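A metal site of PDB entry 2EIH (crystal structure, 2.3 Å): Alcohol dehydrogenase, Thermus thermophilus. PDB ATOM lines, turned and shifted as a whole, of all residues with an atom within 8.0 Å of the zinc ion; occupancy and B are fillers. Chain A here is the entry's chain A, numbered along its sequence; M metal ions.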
ATOM      1  N   LEU A  91      35.733  -0.346  -1.423  1.00  0.00           N
ATOM      2  CA  LEU A  91      35.415  -1.744  -1.681  1.00  0.00           C
ATOM      3  C   LEU A  91      34.141  -2.190  -0.964  1.00  0.00           C
ATOM      4  O   LEU A  91      34.003  -2.048   0.254  1.00  0.00           O
ATOM      5  CB  LEU A  91      36.569  -2.649  -1.253  1.00  0.00           C
ATOM      6  CG  LEU A  91      37.809  -2.636  -2.145  1.00  0.00           C
ATOM      7  CD1 LEU A  91      38.365  -1.227  -2.213  1.00  0.00           C
ATOM      8  CD2 LEU A  91      38.842  -3.596  -1.588  1.00  0.00           C
ATOM      9  N   SER A  92      33.213  -2.745  -1.726  1.00  0.00           N
ATOM     10  CA  SER A  92      31.944  -3.214  -1.198  1.00  0.00           C
ATOM     11  C   SER A  92      31.567  -4.518  -1.897  1.00  0.00           C
ATOM     12  O   SER A  92      32.281  -4.976  -2.791  1.00  0.00           O
ATOM     13  CB  SER A  92      30.860  -2.147  -1.435  1.00  0.00           C
ATOM     14  OG  SER A  92      30.818  -1.778  -2.805  1.00  0.00           O
ATOM     15  N   CYS A  93      30.439  -5.111  -1.497  1.00  0.00           N
ATOM     16  CA  CYS A  93      30.010  -6.374  -2.109  1.00  0.00           C
ATOM     17  C   CYS A  93      29.162  -6.178  -3.362  1.00  0.00           C
ATOM     18  O   CYS A  93      28.969  -7.117  -4.138  1.00  0.00           O
ATOM     19  CB  CYS A  93      29.246  -7.224  -1.098  1.00  0.00           C
ATOM     20  SG  CYS A  93      27.619  -6.576  -0.620  1.00  0.00           S
ATOM     21  N   GLY A  94      28.662  -4.961  -3.539  1.00  0.00           N
ATOM     22  CA  GLY A  94      27.844  -4.655  -4.707  1.00  0.00           C
ATOM     23  C   GLY A  94      26.617  -5.536  -4.897  1.00  0.00           C
ATOM     24  O   GLY A  94      26.147  -5.725  -6.023  1.00  0.00           O
ATOM     25  N   ARG A  95      26.076  -6.068  -3.799  1.00  0.00           N
ATOM     26  CA  ARG A  95      24.893  -6.918  -3.876  1.00  0.00           C
ATOM     27  C   ARG A  95      23.857  -6.622  -2.791  1.00  0.00           C
ATOM     28  O   ARG A  95      22.702  -7.052  -2.899  1.00  0.00           O
ATOM     29  CB  ARG A  95      25.300  -8.385  -3.806  1.00  0.00           C
ATOM     30  CG  ARG A  95      26.305  -8.790  -4.859  1.00  0.00           C
ATOM     31  CD  ARG A  95      26.211 -10.264  -5.167  1.00  0.00           C
ATOM     32  NE  ARG A  95      26.304 -11.077  -3.965  1.00  0.00           N
ATOM     33  CZ  ARG A  95      27.378 -11.144  -3.181  1.00  0.00           C
ATOM     34  NH1 ARG A  95      28.460 -10.448  -3.485  1.00  0.00           N
ATOM     35  NH2 ARG A  95      27.370 -11.906  -2.093  1.00  0.00           N
ATOM     36  N   CYS A  96      24.255  -5.882  -1.754  1.00  0.00           N
ATOM     37  CA  CYS A  96      23.327  -5.548  -0.664  1.00  0.00           C
ATOM     38  C   CYS A  96      22.525  -4.298  -1.022  1.00  0.00           C
ATOM     39  O   CYS A  96      22.850  -3.599  -1.983  1.00  0.00           O
ATOM     40  CB  CYS A  96      24.089  -5.321   0.639  1.00  0.00           C
ATOM     41  SG  CYS A  96      24.895  -3.723   0.771  1.00  0.00           S
ATOM     42  N   GLU A  97      21.499  -4.027  -0.234  1.00  0.00           N
ATOM     43  CA  GLU A  97      20.642  -2.864  -0.444  1.00  0.00           C
ATOM     44  C   GLU A  97      21.481  -1.571  -0.538  1.00  0.00           C
ATOM     45  O   GLU A  97      21.354  -0.813  -1.500  1.00  0.00           O
ATOM     46  CB  GLU A  97      19.618  -2.747   0.691  1.00  0.00           C
ATOM     47  CG  GLU A  97      18.439  -1.810   0.418  1.00  0.00           C
ATOM     48  CD  GLU A  97      17.457  -1.743   1.587  1.00  0.00           C
ATOM     49  OE1 GLU A  97      17.211  -2.788   2.224  1.00  0.00           O
ATOM     50  OE2 GLU A  97      16.928  -0.638   1.858  1.00  0.00           O
ATOM     51  N   ARG A  98      22.338  -1.340   0.453  1.00  0.00           N
ATOM     52  CA  ARG A  98      23.177  -0.145   0.464  1.00  0.00           C
ATOM     53  C   ARG A  98      23.984   0.019  -0.836  1.00  0.00           C
ATOM     54  O   ARG A  98      24.057   1.119  -1.395  1.00  0.00           O
ATOM     55  CB  ARG A  98      24.115  -0.173   1.664  1.00  0.00           C
ATOM     56  CG  ARG A  98      23.440   0.140   2.988  1.00  0.00           C
ATOM     57  CD  ARG A  98      22.786   1.512   2.936  1.00  0.00           C
ATOM     58  NE  ARG A  98      22.542   2.048   4.272  1.00  0.00           N
ATOM     59  CZ  ARG A  98      22.058   3.261   4.516  1.00  0.00           C
ATOM     60  NH1 ARG A  98      21.886   3.674   5.763  1.00  0.00           N
ATOM     61  NH2 ARG A  98      21.754   4.071   3.507  1.00  0.00           N
ATOM     62  N   CYS A  99      24.567  -1.079  -1.312  1.00  0.00           N
ATOM     63  CA  CYS A  99      25.349  -1.043  -2.550  1.00  0.00           C
ATOM     64  C   CYS A  99      24.512  -0.778  -3.788  1.00  0.00           C
ATOM     65  O   CYS A  99      24.896   0.032  -4.633  1.00  0.00           O
ATOM     66  CB  CYS A  99      26.118  -2.351  -2.740  1.00  0.00           C
ATOM     67  SG  CYS A  99      27.629  -2.433  -1.784  1.00  0.00           S
ATOM     68  N   LEU A 100      23.374  -1.459  -3.915  1.00  0.00           N
ATOM     69  CA  LEU A 100      22.527  -1.232  -5.089  1.00  0.00           C
ATOM     70  C   LEU A 100      21.943   0.178  -5.123  1.00  0.00           C
ATOM     71  O   LEU A 100      21.481   0.620  -6.165  1.00  0.00           O
ATOM     72  CB  LEU A 100      21.391  -2.263  -5.157  1.00  0.00           C
ATOM     73  CG  LEU A 100      21.699  -3.639  -5.772  1.00  0.00           C
ATOM     74  CD1 LEU A 100      22.828  -3.536  -6.797  1.00  0.00           C
ATOM     75  CD2 LEU A 100      22.057  -4.628  -4.702  1.00  0.00           C
ATOM     76  N   GLU A 103      25.107   3.758  -2.200  1.00  0.00           N
ATOM     77  CA  GLU A 103      25.734   4.027  -0.911  1.00  0.00           C
ATOM     78  C   GLU A 103      26.686   2.906  -0.503  1.00  0.00           C
ATOM     79  O   GLU A 103      26.589   2.365   0.601  1.00  0.00           O
ATOM     80  CB  GLU A 103      24.663   4.214   0.159  1.00  0.00           C
ATOM     81  CG  GLU A 103      23.762   5.438  -0.048  1.00  0.00           C
ATOM     82  CD  GLU A 103      22.381   5.232   0.533  1.00  0.00           C
ATOM     83  OE1 GLU A 103      21.552   6.176   0.459  1.00  0.00           O
ATOM     84  OE2 GLU A 103      22.104   4.125   1.061  1.00  0.00           O
ATOM     85  N   ASP A 104      27.624   2.565  -1.378  1.00  0.00           N
ATOM     86  CA  ASP A 104      28.573   1.501  -1.095  1.00  0.00           C
ATOM     87  C   ASP A 104      29.395   1.757   0.172  1.00  0.00           C
ATOM     88  O   ASP A 104      29.706   0.823   0.922  1.00  0.00           O
ATOM     89  CB  ASP A 104      29.499   1.295  -2.312  1.00  0.00           C
ATOM     90  CG  ASP A 104      30.312   2.535  -2.646  1.00  0.00           C
ATOM     91  OD1 ASP A 104      29.720   3.592  -2.894  1.00  0.00           O
ATOM     92  OD2 ASP A 104      31.556   2.432  -2.658  1.00  0.00           O
ATOM     93  N   ASN A 105      29.728   3.025   0.422  1.00  0.00           N
ATOM     94  CA  ASN A 105      30.502   3.400   1.601  1.00  0.00           C
ATOM     95  C   ASN A 105      29.724   3.164   2.895  1.00  0.00           C
ATOM     96  O   ASN A 105      30.225   3.403   3.991  1.00  0.00           O
ATOM     97  CB  ASN A 105      30.963   4.880   1.507  1.00  0.00           C
ATOM     98  CG  ASN A 105      29.806   5.861   1.487  1.00  0.00           C
ATOM     99  OD1 ASN A 105      28.843   5.697   0.744  1.00  0.00           O
ATOM    100  ND2 ASN A 105      29.901   6.903   2.308  1.00  0.00           N
ATOM    101  N   LEU A 106      28.486   2.705   2.744  1.00  0.00           N
ATOM    102  CA  LEU A 106      27.648   2.398   3.900  1.00  0.00           C
ATOM    103  C   LEU A 106      27.334   0.904   3.930  1.00  0.00           C
ATOM    104  O   LEU A 106      26.509   0.442   4.719  1.00  0.00           O
ATOM    105  CB  LEU A 106      26.350   3.222   3.882  1.00  0.00           C
ATOM    106  CG  LEU A 106      26.366   4.584   4.596  1.00  0.00           C
ATOM    107  CD1 LEU A 106      26.626   4.383   6.092  1.00  0.00           C
ATOM    108  CD2 LEU A 106      27.463   5.464   3.993  1.00  0.00           C
ATOM    109  N   CYS A 107      27.996   0.158   3.057  1.00  0.00           N
ATOM    110  CA  CYS A 107      27.810  -1.290   2.988  1.00  0.00           C
ATOM    111  C   CYS A 107      28.295  -1.918   4.296  1.00  0.00           C
ATOM    112  O   CYS A 107      29.281  -1.477   4.885  1.00  0.00           O
ATOM    113  CB  CYS A 107      28.621  -1.874   1.829  1.00  0.00           C
ATOM    114  SG  CYS A 107      28.837  -3.677   1.886  1.00  0.00           S
ATOM    115  N   PRO A 108      27.586  -2.948   4.776  1.00  0.00           N
ATOM    116  CA  PRO A 108      28.013  -3.576   6.025  1.00  0.00           C
ATOM    117  C   PRO A 108      29.399  -4.234   5.886  1.00  0.00           C
ATOM    118  O   PRO A 108      30.118  -4.391   6.879  1.00  0.00           O
ATOM    119  CB  PRO A 108      26.896  -4.582   6.304  1.00  0.00           C
ATOM    120  CG  PRO A 108      26.379  -4.914   4.928  1.00  0.00           C
ATOM    121  CD  PRO A 108      26.355  -3.574   4.251  1.00  0.00           C
ATOM    122  N   ARG A 109      29.770  -4.591   4.660  1.00  0.00           N
ATOM    123  CA  ARG A 109      31.060  -5.229   4.357  1.00  0.00           C
ATOM    124  C   ARG A 109      32.047  -4.248   3.701  1.00  0.00           C
ATOM    125  O   ARG A 109      33.074  -4.655   3.157  1.00  0.00           O
ATOM    126  CB  ARG A 109      30.864  -6.421   3.411  1.00  0.00           C
ATOM    127  CG  ARG A 109      30.117  -7.608   4.031  1.00  0.00           C
ATOM    128  CD  ARG A 109      30.988  -8.338   5.053  1.00  0.00           C
ATOM    129  NE  ARG A 109      30.271  -9.373   5.817  1.00  0.00           N
ATOM    130  CZ  ARG A 109      29.401  -9.121   6.792  1.00  0.00           C
ATOM    131  NH1 ARG A 109      28.801 -10.130   7.417  1.00  0.00           N
ATOM    132  NH2 ARG A 109      29.136  -7.870   7.150  1.00  0.00           N
ATOM    133  N   TYR A 110      31.718  -2.960   3.772  1.00  0.00           N
ATOM    134  CA  TYR A 110      32.537  -1.914   3.181  1.00  0.00           C
ATOM    135  C   TYR A 110      33.973  -1.963   3.671  1.00  0.00           C
ATOM    136  O   TYR A 110      34.230  -2.128   4.866  1.00  0.00           O
ATOM    137  CB  TYR A 110      31.962  -0.548   3.500  1.00  0.00           C
ATOM    138  CG  TYR A 110      32.666   0.588   2.790  1.00  0.00           C
ATOM    139  CD1 TYR A 110      33.198   1.650   3.504  1.00  0.00           C
ATOM    140  CD2 TYR A 110      32.751   0.614   1.394  1.00  0.00           C
ATOM    141  CE1 TYR A 110      33.816   2.719   2.868  1.00  0.00           C
ATOM    142  CE2 TYR A 110      33.354   1.663   0.732  1.00  0.00           C
ATOM    143  CZ  TYR A 110      33.878   2.725   1.474  1.00  0.00           C
ATOM    144  OH  TYR A 110      34.442   3.805   0.823  1.00  0.00           O
ATOM    145  N   LYS A 294      31.239   5.607  -4.669  1.00  0.00           N
ATOM    146  CA  LYS A 294      32.178   5.432  -5.766  1.00  0.00           C
ATOM    147  C   LYS A 294      31.809   6.229  -7.003  1.00  0.00           C
ATOM    148  O   LYS A 294      32.676   6.661  -7.759  1.00  0.00           O
ATOM    149  CB  LYS A 294      32.271   3.954  -6.149  1.00  0.00           C
ATOM    150  CG  LYS A 294      33.097   3.113  -5.239  1.00  0.00           C
ATOM    151  CD  LYS A 294      33.434   1.785  -5.906  1.00  0.00           C
ATOM    152  CE  LYS A 294      32.336   0.749  -5.672  1.00  0.00           C
ATOM    153  NZ  LYS A 294      32.281   0.343  -4.246  1.00  0.00           N
HETATM  154 ZN    ZN M   1      27.241  -4.180  -0.131  1.00  0.00          ZN
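The zinc ion is bound by the side-chain sulfur (SG) of Cys 99 (2.4 Å), the side-chain sulfur (SG) of Cys 93 (2.5 Å), the side-chain sulfur (SG) of Cys 96 (2.6 Å) and the side-chain sulfur (SG) of Cys 107 (2.6 Å).
Gly 94 touches the zinc ion (N to ZN, 3.8 Å).
Within 4 Å of the zinc ion: Cys 93, Gly 94, Cys 96, Cys 99 and Cys 107.
The backbone NH (N) of Tyr 110 lies close to the side-chain sulfur (SG) of Cys 107 (3.5 Å).
SG of Cys 99 sits close to OG of Ser 92 (3.4 Å).
The backbone NH of Arg 98 sits close to the side-chain sulfur of Cys 96 (3.5 Å).
The backbone carbonyl oxygen (O) of Cys 93 lies close to the guanidinium group (NH1) of Arg 95 (3.4 Å).
SG of Cys 99 sits close to N of Gly 94, at 3.2 Å.
The side-chain sulfur (SG) of Cys 107 lies close to the backbone NH (N) of Arg 109 (3.1 Å).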
